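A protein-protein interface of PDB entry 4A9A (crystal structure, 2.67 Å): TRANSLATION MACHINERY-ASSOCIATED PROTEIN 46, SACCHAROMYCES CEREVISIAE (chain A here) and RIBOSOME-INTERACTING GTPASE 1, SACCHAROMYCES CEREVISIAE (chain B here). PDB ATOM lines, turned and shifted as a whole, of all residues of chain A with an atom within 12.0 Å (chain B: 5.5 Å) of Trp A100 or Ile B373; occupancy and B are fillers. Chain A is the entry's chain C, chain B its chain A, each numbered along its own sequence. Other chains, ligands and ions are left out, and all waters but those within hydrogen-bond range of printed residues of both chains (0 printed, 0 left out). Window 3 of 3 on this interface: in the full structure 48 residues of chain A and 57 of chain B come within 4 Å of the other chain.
The backbone NH (N) of Lys B376 sits at hydrogen-bond distance from the backbone carbonyl oxygen (O) of Asp B341. O of Leu B374 sits at hydrogen-bond distance from N of Arg B343 (2.9 Å). The backbone NH (N) of Leu B374 lies within hydrogen-bond range of the backbone carbonyl oxygen (O) of Asn B344 (2.8 Å).
O of Leu B338 touches CH2 of Trp A100 (3.3 Å). CZ3 of Trp A100 touches O of Asp B341, at 3.5 Å. Ile B373 touches Trp A100. Leu B374 touches Trp A100. Lys B375 touches Trp A100.
Of chain B, only Leu B338, Asp B341, Ile B373, Leu B374 and Lys B375 come within 4 Å of Trp A100. Leu A102 touches none of the printed residues of chain B. No residue of chain A comes within 4 Å of Phe B330. No residue of chain A comes within 4 Å of Cys B331. Asp B341 touches one residue of chain A. No residue of chain A comes within 4 Å of Phe B342. No residue of chain A comes within 4 Å of Val B371. The nearest residue of chain B that does not touch Trp A100 is Phe B342 (4.1 Å).
Printed residues of chain A that touch a printed residue of chain B: Trp A100. Of the 18 printed residues of chain B, 5 touch a printed residue of chain A. Printed residues of chain B that touch a printed residue of chain A: Leu B338, Asp B341, Ile B373, Leu B374 and Lys B375. Hydrophobic or aromatic side chains of chain B that line the printed part of chain A: Leu B338 and Ile B373. Among the printed residues, 5 pairs touch across the chains. Among the printed residues, no Asp or Glu carboxylate lies within 4 Å of a Lys or Arg side-chain nitrogen of the other chain.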
ATOM      1  N   ALA A  99     -20.682  15.526  36.079  1.00  0.00           N
ATOM      2  CA  ALA A  99     -19.980  16.764  36.381  1.00  0.00           C
ATOM      3  C   ALA A  99     -18.632  16.807  35.660  1.00  0.00           C
ATOM      4  O   ALA A  99     -17.775  15.939  35.861  1.00  0.00           O
ATOM      5  CB  ALA A  99     -19.795  16.917  37.883  1.00  0.00           C
ATOM      6  N   TRP A 100     -18.446  17.828  34.827  1.00  0.00           N
ATOM      7  CA  TRP A 100     -17.277  17.906  33.953  1.00  0.00           C
ATOM      8  C   TRP A 100     -16.365  19.056  34.299  1.00  0.00           C
ATOM      9  O   TRP A 100     -16.755  20.222  34.206  1.00  0.00           O
ATOM     10  CB  TRP A 100     -17.730  18.020  32.498  1.00  0.00           C
ATOM     11  CG  TRP A 100     -16.728  17.524  31.479  1.00  0.00           C
ATOM     12  CD1 TRP A 100     -15.349  17.373  31.634  1.00  0.00           C
ATOM     13  CD2 TRP A 100     -16.997  17.128  30.088  1.00  0.00           C
ATOM     14  NE1 TRP A 100     -14.772  16.910  30.480  1.00  0.00           N
ATOM     15  CE2 TRP A 100     -15.702  16.743  29.512  1.00  0.00           C
ATOM     16  CE3 TRP A 100     -18.137  17.053  29.295  1.00  0.00           C
ATOM     17  CZ2 TRP A 100     -15.582  16.303  28.201  1.00  0.00           C
ATOM     18  CZ3 TRP A 100     -18.004  16.607  27.974  1.00  0.00           C
ATOM     19  CH2 TRP A 100     -16.755  16.242  27.442  1.00  0.00           C
ATOM     20  N   ASP A 101     -15.133  18.732  34.690  1.00  0.00           N
ATOM     21  CA  ASP A 101     -14.124  19.739  35.017  1.00  0.00           C
ATOM     22  C   ASP A 101     -13.403  20.210  33.748  1.00  0.00           C
ATOM     23  O   ASP A 101     -12.488  19.545  33.250  1.00  0.00           O
ATOM     24  CB  ASP A 101     -13.129  19.187  36.056  1.00  0.00           C
ATOM     25  CG  ASP A 101     -11.966  20.145  36.350  1.00  0.00           C
ATOM     26  OD1 ASP A 101     -12.172  21.377  36.390  1.00  0.00           O
ATOM     27  OD2 ASP A 101     -10.837  19.655  36.557  1.00  0.00           O
ATOM     28  N   LEU A 102     -13.822  21.360  33.232  1.00  0.00           N
ATOM     29  CA  LEU A 102     -13.259  21.883  31.991  1.00  0.00           C
ATOM     30  C   LEU A 102     -12.131  22.905  32.194  1.00  0.00           C
ATOM     31  O   LEU A 102     -11.497  23.333  31.225  1.00  0.00           O
ATOM     32  CB  LEU A 102     -14.369  22.440  31.096  1.00  0.00           C
ATOM     33  CG  LEU A 102     -15.585  23.103  31.746  1.00  0.00           C
ATOM     34  CD1 LEU A 102     -15.229  24.386  32.490  1.00  0.00           C
ATOM     35  CD2 LEU A 102     -16.617  23.380  30.669  1.00  0.00           C
ATOM     36  N   THR A 103     -11.873  23.261  33.454  1.00  0.00           N
ATOM     37  CA  THR A 103     -10.845  24.246  33.836  1.00  0.00           C
ATOM     38  C   THR A 103      -9.624  24.269  32.914  1.00  0.00           C
ATOM     39  O   THR A 103      -9.295  25.318  32.359  1.00  0.00           O
ATOM     40  CB  THR A 103     -10.375  24.055  35.299  1.00  0.00           C
ATOM     41  OG1 THR A 103     -11.516  23.992  36.161  1.00  0.00           O
ATOM     42  CG2 THR A 103      -9.469  25.209  35.748  1.00  0.00           C
ATOM     43  N   GLU A 104      -8.974  23.115  32.753  1.00  0.00           N
ATOM     44  CA  GLU A 104      -7.749  22.996  31.951  1.00  0.00           C
ATOM     45  C   GLU A 104      -7.921  23.516  30.520  1.00  0.00           C
ATOM     46  O   GLU A 104      -7.047  24.214  29.995  1.00  0.00           O
ATOM     47  CB  GLU A 104      -7.245  21.556  31.946  1.00  0.00           C
ATOM     48  N   PHE A 105      -9.058  23.189  29.907  1.00  0.00           N
ATOM     49  CA  PHE A 105      -9.339  23.591  28.531  1.00  0.00           C
ATOM     50  C   PHE A 105      -9.726  25.063  28.432  1.00  0.00           C
ATOM     51  O   PHE A 105      -9.262  25.764  27.527  1.00  0.00           O
ATOM     52  CB  PHE A 105     -10.416  22.696  27.913  1.00  0.00           C
ATOM     53  CG  PHE A 105     -10.132  21.224  28.050  1.00  0.00           C
ATOM     54  CD1 PHE A 105      -9.127  20.618  27.297  1.00  0.00           C
ATOM     55  CD2 PHE A 105     -10.866  20.440  28.934  1.00  0.00           C
ATOM     56  CE1 PHE A 105      -8.867  19.260  27.427  1.00  0.00           C
ATOM     57  CE2 PHE A 105     -10.605  19.082  29.071  1.00  0.00           C
ATOM     58  CZ  PHE A 105      -9.609  18.491  28.314  1.00  0.00           C
ATOM     59  N   THR A 106     -10.558  25.527  29.365  1.00  0.00           N
ATOM     60  CA  THR A 106     -10.959  26.937  29.411  1.00  0.00           C
ATOM     61  C   THR A 106      -9.777  27.860  29.719  1.00  0.00           C
ATOM     62  O   THR A 106      -9.545  28.819  28.994  1.00  0.00           O
ATOM     63  CB  THR A 106     -12.106  27.207  30.412  1.00  0.00           C
ATOM     64  OG1 THR A 106     -11.730  26.742  31.712  1.00  0.00           O
ATOM     65  CG2 THR A 106     -13.394  26.526  29.963  1.00  0.00           C
ATOM     66  N   ASP A 107      -9.025  27.567  30.778  1.00  0.00           N
ATOM     67  CA  ASP A 107      -7.841  28.362  31.116  1.00  0.00           C
ATOM     68  C   ASP A 107      -6.994  28.578  29.876  1.00  0.00           C
ATOM     69  O   ASP A 107      -6.611  29.707  29.577  1.00  0.00           O
ATOM     70  CB  ASP A 107      -7.006  27.690  32.216  1.00  0.00           C
ATOM     71  CG  ASP A 107      -7.583  27.903  33.609  1.00  0.00           C
ATOM     72  OD1 ASP A 107      -8.825  27.921  33.766  1.00  0.00           O
ATOM     73  OD2 ASP A 107      -6.786  28.040  34.558  1.00  0.00           O
ATOM     74  N   LEU A 109      -7.902  28.334  26.767  1.00  0.00           N
ATOM     75  CA  LEU A 109      -8.648  29.029  25.737  1.00  0.00           C
ATOM     76  C   LEU A 109      -8.581  30.539  25.917  1.00  0.00           C
ATOM     77  O   LEU A 109      -8.343  31.261  24.948  1.00  0.00           O
ATOM     78  CB  LEU A 109     -10.108  28.548  25.727  1.00  0.00           C
ATOM     79  CG  LEU A 109     -11.103  28.888  24.604  1.00  0.00           C
ATOM     80  CD1 LEU A 109     -11.928  30.136  24.911  1.00  0.00           C
ATOM     81  CD2 LEU A 109     -10.457  28.967  23.223  1.00  0.00           C
ATOM     82  N   LYS A 110      -8.803  31.017  27.142  1.00  0.00           N
ATOM     83  CA  LYS A 110      -8.744  32.455  27.415  1.00  0.00           C
ATOM     84  C   LYS A 110      -7.304  32.972  27.357  1.00  0.00           C
ATOM     85  O   LYS A 110      -7.061  34.109  26.949  1.00  0.00           O
ATOM     86  CB  LYS A 110      -9.451  32.838  28.725  1.00  0.00           C
ATOM     87  CG  LYS A 110      -9.074  32.020  29.953  1.00  0.00           C
ATOM     88  CD  LYS A 110      -9.845  32.463  31.197  1.00  0.00           C
ATOM     89  CE  LYS A 110     -11.252  31.874  31.282  1.00  0.00           C
ATOM     90  NZ  LYS A 110     -11.291  30.586  32.030  1.00  0.00           N
ATOM     91  N   LYS B 306     -20.600  27.734  33.082  1.00  0.00           N
ATOM     92  CA  LYS B 306     -20.889  27.527  34.497  1.00  0.00           C
ATOM     93  C   LYS B 306     -20.519  26.105  34.880  1.00  0.00           C
ATOM     94  O   LYS B 306     -21.057  25.157  34.310  1.00  0.00           O
ATOM     95  CB  LYS B 306     -22.373  27.759  34.774  1.00  0.00           C
ATOM     96  CG  LYS B 306     -22.778  27.533  36.217  1.00  0.00           C
ATOM     97  CD  LYS B 306     -24.289  27.513  36.392  1.00  0.00           C
ATOM     98  CE  LYS B 306     -24.674  27.135  37.817  1.00  0.00           C
ATOM     99  NZ  LYS B 306     -24.324  25.720  38.116  1.00  0.00           N
ATOM    100  N   PHE B 330     -20.255  25.319  20.420  1.00  0.00           N
ATOM    101  CA  PHE B 330     -19.727  25.722  21.714  1.00  0.00           C
ATOM    102  C   PHE B 330     -18.631  24.766  22.164  1.00  0.00           C
ATOM    103  O   PHE B 330     -17.520  25.201  22.496  1.00  0.00           O
ATOM    104  CB  PHE B 330     -20.850  25.744  22.734  1.00  0.00           C
ATOM    105  CG  PHE B 330     -20.400  26.013  24.134  1.00  0.00           C
ATOM    106  CD1 PHE B 330     -19.861  27.240  24.484  1.00  0.00           C
ATOM    107  CD2 PHE B 330     -20.535  25.048  25.111  1.00  0.00           C
ATOM    108  CE1 PHE B 330     -19.452  27.497  25.778  1.00  0.00           C
ATOM    109  CE2 PHE B 330     -20.135  25.303  26.413  1.00  0.00           C
ATOM    110  CZ  PHE B 330     -19.595  26.533  26.747  1.00  0.00           C
ATOM    111  N   CYS B 331     -18.940  23.467  22.136  1.00  0.00           N
ATOM    112  CA  CYS B 331     -17.996  22.428  22.541  1.00  0.00           C
ATOM    113  C   CYS B 331     -16.689  22.536  21.772  1.00  0.00           C
ATOM    114  O   CYS B 331     -15.605  22.596  22.366  1.00  0.00           O
ATOM    115  CB  CYS B 331     -18.607  21.035  22.355  1.00  0.00           C
ATOM    116  SG  CYS B 331     -19.948  20.618  23.512  1.00  0.00           S
ATOM    117  N   ILE B 334     -14.351  25.268  22.558  1.00  0.00           N
ATOM    118  CA  ILE B 334     -13.596  25.071  23.797  1.00  0.00           C
ATOM    119  C   ILE B 334     -12.464  24.053  23.639  1.00  0.00           C
ATOM    120  O   ILE B 334     -11.345  24.298  24.086  1.00  0.00           O
ATOM    121  CB  ILE B 334     -14.519  24.714  24.984  1.00  0.00           C
ATOM    122  CG1 ILE B 334     -15.496  25.866  25.231  1.00  0.00           C
ATOM    123  CG2 ILE B 334     -13.702  24.403  26.236  1.00  0.00           C
ATOM    124  CD1 ILE B 334     -16.301  25.751  26.505  1.00  0.00           C
ATOM    125  N   LEU B 338     -14.197  17.265  23.199  1.00  0.00           N
ATOM    126  CA  LEU B 338     -15.440  17.290  23.998  1.00  0.00           C
ATOM    127  C   LEU B 338     -16.649  16.539  23.436  1.00  0.00           C
ATOM    128  O   LEU B 338     -17.375  15.895  24.192  1.00  0.00           O
ATOM    129  CB  LEU B 338     -15.831  18.736  24.320  1.00  0.00           C
ATOM    130  CG  LEU B 338     -15.340  19.379  25.623  1.00  0.00           C
ATOM    131  CD1 LEU B 338     -14.000  18.850  26.114  1.00  0.00           C
ATOM    132  CD2 LEU B 338     -15.270  20.884  25.439  1.00  0.00           C
ATOM    133  N   VAL B 339     -16.858  16.631  22.124  1.00  0.00           N
ATOM    134  CA  VAL B 339     -17.975  15.970  21.434  1.00  0.00           C
ATOM    135  C   VAL B 339     -18.012  14.457  21.690  1.00  0.00           C
ATOM    136  O   VAL B 339     -19.086  13.871  21.866  1.00  0.00           O
ATOM    137  CB  VAL B 339     -17.931  16.263  19.913  1.00  0.00           C
ATOM    138  CG1 VAL B 339     -18.872  15.350  19.136  1.00  0.00           C
ATOM    139  CG2 VAL B 339     -18.267  17.721  19.647  1.00  0.00           C
ATOM    140  N   ASP B 341     -17.114  12.696  24.257  1.00  0.00           N
ATOM    141  CA  ASP B 341     -17.537  12.292  25.599  1.00  0.00           C
ATOM    142  C   ASP B 341     -18.710  13.130  26.112  1.00  0.00           C
ATOM    143  O   ASP B 341     -18.896  13.292  27.321  1.00  0.00           O
ATOM    144  CB  ASP B 341     -16.361  12.371  26.579  1.00  0.00           C
ATOM    145  CG  ASP B 341     -15.101  11.715  26.044  1.00  0.00           C
ATOM    146  OD1 ASP B 341     -15.137  10.514  25.689  1.00  0.00           O
ATOM    147  OD2 ASP B 341     -14.067  12.411  25.977  1.00  0.00           O
ATOM    148  N   PHE B 342     -19.502  13.654  25.186  1.00  0.00           N
ATOM    149  CA  PHE B 342     -20.620  14.522  25.521  1.00  0.00           C
ATOM    150  C   PHE B 342     -21.831  13.698  25.916  1.00  0.00           C
ATOM    151  O   PHE B 342     -22.304  12.892  25.121  1.00  0.00           O
ATOM    152  CB  PHE B 342     -20.959  15.377  24.305  1.00  0.00           C
ATOM    153  CG  PHE B 342     -22.189  16.229  24.465  1.00  0.00           C
ATOM    154  CD1 PHE B 342     -22.096  17.516  24.992  1.00  0.00           C
ATOM    155  CD2 PHE B 342     -23.432  15.763  24.046  1.00  0.00           C
ATOM    156  CE1 PHE B 342     -23.219  18.311  25.119  1.00  0.00           C
ATOM    157  CE2 PHE B 342     -24.564  16.555  24.174  1.00  0.00           C
ATOM    158  CZ  PHE B 342     -24.455  17.833  24.704  1.00  0.00           C
ATOM    159  N   ARG B 343     -22.330  13.896  27.135  1.00  0.00           N
ATOM    160  CA  ARG B 343     -23.612  13.300  27.547  1.00  0.00           C
ATOM    161  C   ARG B 343     -24.742  14.242  27.117  1.00  0.00           C
ATOM    162  O   ARG B 343     -25.558  13.897  26.258  1.00  0.00           O
ATOM    163  CB  ARG B 343     -23.626  13.024  29.062  1.00  0.00           C
ATOM    164  CG  ARG B 343     -24.982  12.707  29.685  1.00  0.00           C
ATOM    165  CD  ARG B 343     -25.336  11.228  29.674  1.00  0.00           C
ATOM    166  NE  ARG B 343     -26.710  11.030  30.136  1.00  0.00           N
ATOM    167  CZ  ARG B 343     -27.085  10.248  31.150  1.00  0.00           C
ATOM    168  NH1 ARG B 343     -26.196   9.537  31.843  1.00  0.00           N
ATOM    169  NH2 ARG B 343     -28.369  10.166  31.468  1.00  0.00           N
ATOM    170  N   ASN B 344     -24.756  15.437  27.703  1.00  0.00           N
ATOM    171  CA  ASN B 344     -25.687  16.505  27.336  1.00  0.00           C
ATOM    172  C   ASN B 344     -25.288  17.841  27.976  1.00  0.00           C
ATOM    173  O   ASN B 344     -24.260  17.922  28.659  1.00  0.00           O
ATOM    174  CB  ASN B 344     -27.148  16.130  27.658  1.00  0.00           C
ATOM    175  CG  ASN B 344     -27.346  15.683  29.098  1.00  0.00           C
ATOM    176  OD1 ASN B 344     -26.602  16.077  30.000  1.00  0.00           O
ATOM    177  ND2 ASN B 344     -28.363  14.855  29.319  1.00  0.00           N
ATOM    178  N   ALA B 345     -26.098  18.880  27.751  1.00  0.00           N
ATOM    179  CA  ALA B 345     -25.822  20.214  28.282  1.00  0.00           C
ATOM    180  C   ALA B 345     -27.006  20.814  29.027  1.00  0.00           C
ATOM    181  O   ALA B 345     -28.154  20.715  28.577  1.00  0.00           O
ATOM    182  CB  ALA B 345     -25.394  21.143  27.165  1.00  0.00           C
ATOM    183  N   LEU B 346     -26.711  21.440  30.163  1.00  0.00           N
ATOM    184  CA  LEU B 346     -27.701  22.157  30.937  1.00  0.00           C
ATOM    185  C   LEU B 346     -27.657  23.628  30.570  1.00  0.00           C
ATOM    186  O   LEU B 346     -26.608  24.273  30.658  1.00  0.00           O
ATOM    187  CB  LEU B 346     -27.434  21.986  32.422  1.00  0.00           C
ATOM    188  CG  LEU B 346     -28.586  22.394  33.339  1.00  0.00           C
ATOM    189  CD1 LEU B 346     -29.869  21.673  32.941  1.00  0.00           C
ATOM    190  CD2 LEU B 346     -28.242  22.133  34.802  1.00  0.00           C
ATOM    191  N   VAL B 371     -24.401  27.914  30.210  1.00  0.00           N
ATOM    192  CA  VAL B 371     -24.262  26.502  29.812  1.00  0.00           C
ATOM    193  C   VAL B 371     -23.309  25.665  30.676  1.00  0.00           C
ATOM    194  O   VAL B 371     -22.183  26.081  30.965  1.00  0.00           O
ATOM    195  CB  VAL B 371     -23.824  26.384  28.340  1.00  0.00           C
ATOM    196  CG1 VAL B 371     -23.570  24.930  27.953  1.00  0.00           C
ATOM    197  CG2 VAL B 371     -24.863  27.015  27.423  1.00  0.00           C
ATOM    198  N   THR B 372     -23.778  24.484  31.071  1.00  0.00           N
ATOM    199  CA  THR B 372     -22.980  23.505  31.796  1.00  0.00           C
ATOM    200  C   THR B 372     -22.970  22.206  31.001  1.00  0.00           C
ATOM    201  O   THR B 372     -24.003  21.552  30.882  1.00  0.00           O
ATOM    202  CB  THR B 372     -23.592  23.194  33.177  1.00  0.00           C
ATOM    203  OG1 THR B 372     -23.759  24.404  33.921  1.00  0.00           O
ATOM    204  CG2 THR B 372     -22.700  22.243  33.961  1.00  0.00           C
ATOM    205  N   ILE B 373     -21.819  21.822  30.460  1.00  0.00           N
ATOM    206  CA  ILE B 373     -21.724  20.560  29.723  1.00  0.00           C
ATOM    207  C   ILE B 373     -21.500  19.377  30.662  1.00  0.00           C
ATOM    208  O   ILE B 373     -20.855  19.514  31.704  1.00  0.00           O
ATOM    209  CB  ILE B 373     -20.615  20.598  28.668  1.00  0.00           C
ATOM    210  CG1 ILE B 373     -20.863  21.742  27.696  1.00  0.00           C
ATOM    211  CG2 ILE B 373     -20.567  19.292  27.891  1.00  0.00           C
ATOM    212  CD1 ILE B 373     -19.650  22.035  26.834  1.00  0.00           C
ATOM    213  N   LEU B 374     -22.039  18.215  30.288  1.00  0.00           N
ATOM    214  CA  LEU B 374     -21.932  17.018  31.123  1.00  0.00           C
ATOM    215  C   LEU B 374     -21.267  15.854  30.405  1.00  0.00           C
ATOM    216  O   LEU B 374     -21.439  15.659  29.192  1.00  0.00           O
ATOM    217  CB  LEU B 374     -23.295  16.640  31.693  1.00  0.00           C
ATOM    218  CG  LEU B 374     -23.812  17.839  32.501  1.00  0.00           C
ATOM    219  CD1 LEU B 374     -25.156  18.337  31.983  1.00  0.00           C
ATOM    220  CD2 LEU B 374     -23.807  17.596  34.006  1.00  0.00           C
ATOM    221  N   LYS B 375     -20.507  15.090  31.184  1.00  0.00           N
ATOM    222  CA  LYS B 375     -19.629  14.052  30.669  1.00  0.00           C
ATOM    223  C   LYS B 375     -20.336  12.697  30.572  1.00  0.00           C
ATOM    224  O   LYS B 375     -21.005  12.259  31.513  1.00  0.00           O
ATOM    225  CB  LYS B 375     -18.378  13.951  31.561  1.00  0.00           C
ATOM    226  CG  LYS B 375     -17.198  13.216  30.943  1.00  0.00           C
ATOM    227  CD  LYS B 375     -15.951  13.311  31.815  1.00  0.00           C
ATOM    228  CE  LYS B 375     -14.715  12.872  31.041  1.00  0.00           C
ATOM    229  NZ  LYS B 375     -13.456  13.048  31.816  1.00  0.00           N
ATOM    230  N   LYS B 376     -20.166  12.050  29.419  1.00  0.00           N
ATOM    231  CA  LYS B 376     -20.670  10.700  29.163  1.00  0.00           C
ATOM    232  C   LYS B 376     -19.901   9.695  30.001  1.00  0.00           C
ATOM    233  O   LYS B 376     -20.127   9.588  31.202  1.00  0.00           O
ATOM    234  CB  LYS B 376     -20.540  10.341  27.674  1.00  0.00           C
ATOM    235  CG  LYS B 376     -21.777   9.663  27.095  1.00  0.00           C
ATOM    236  CD  LYS B 376     -21.491   8.862  25.830  1.00  0.00           C
ATOM    237  CE  LYS B 376     -22.665   7.937  25.518  1.00  0.00           C
ATOM    238  NZ  LYS B 376     -22.281   6.695  24.786  1.00  0.00           N
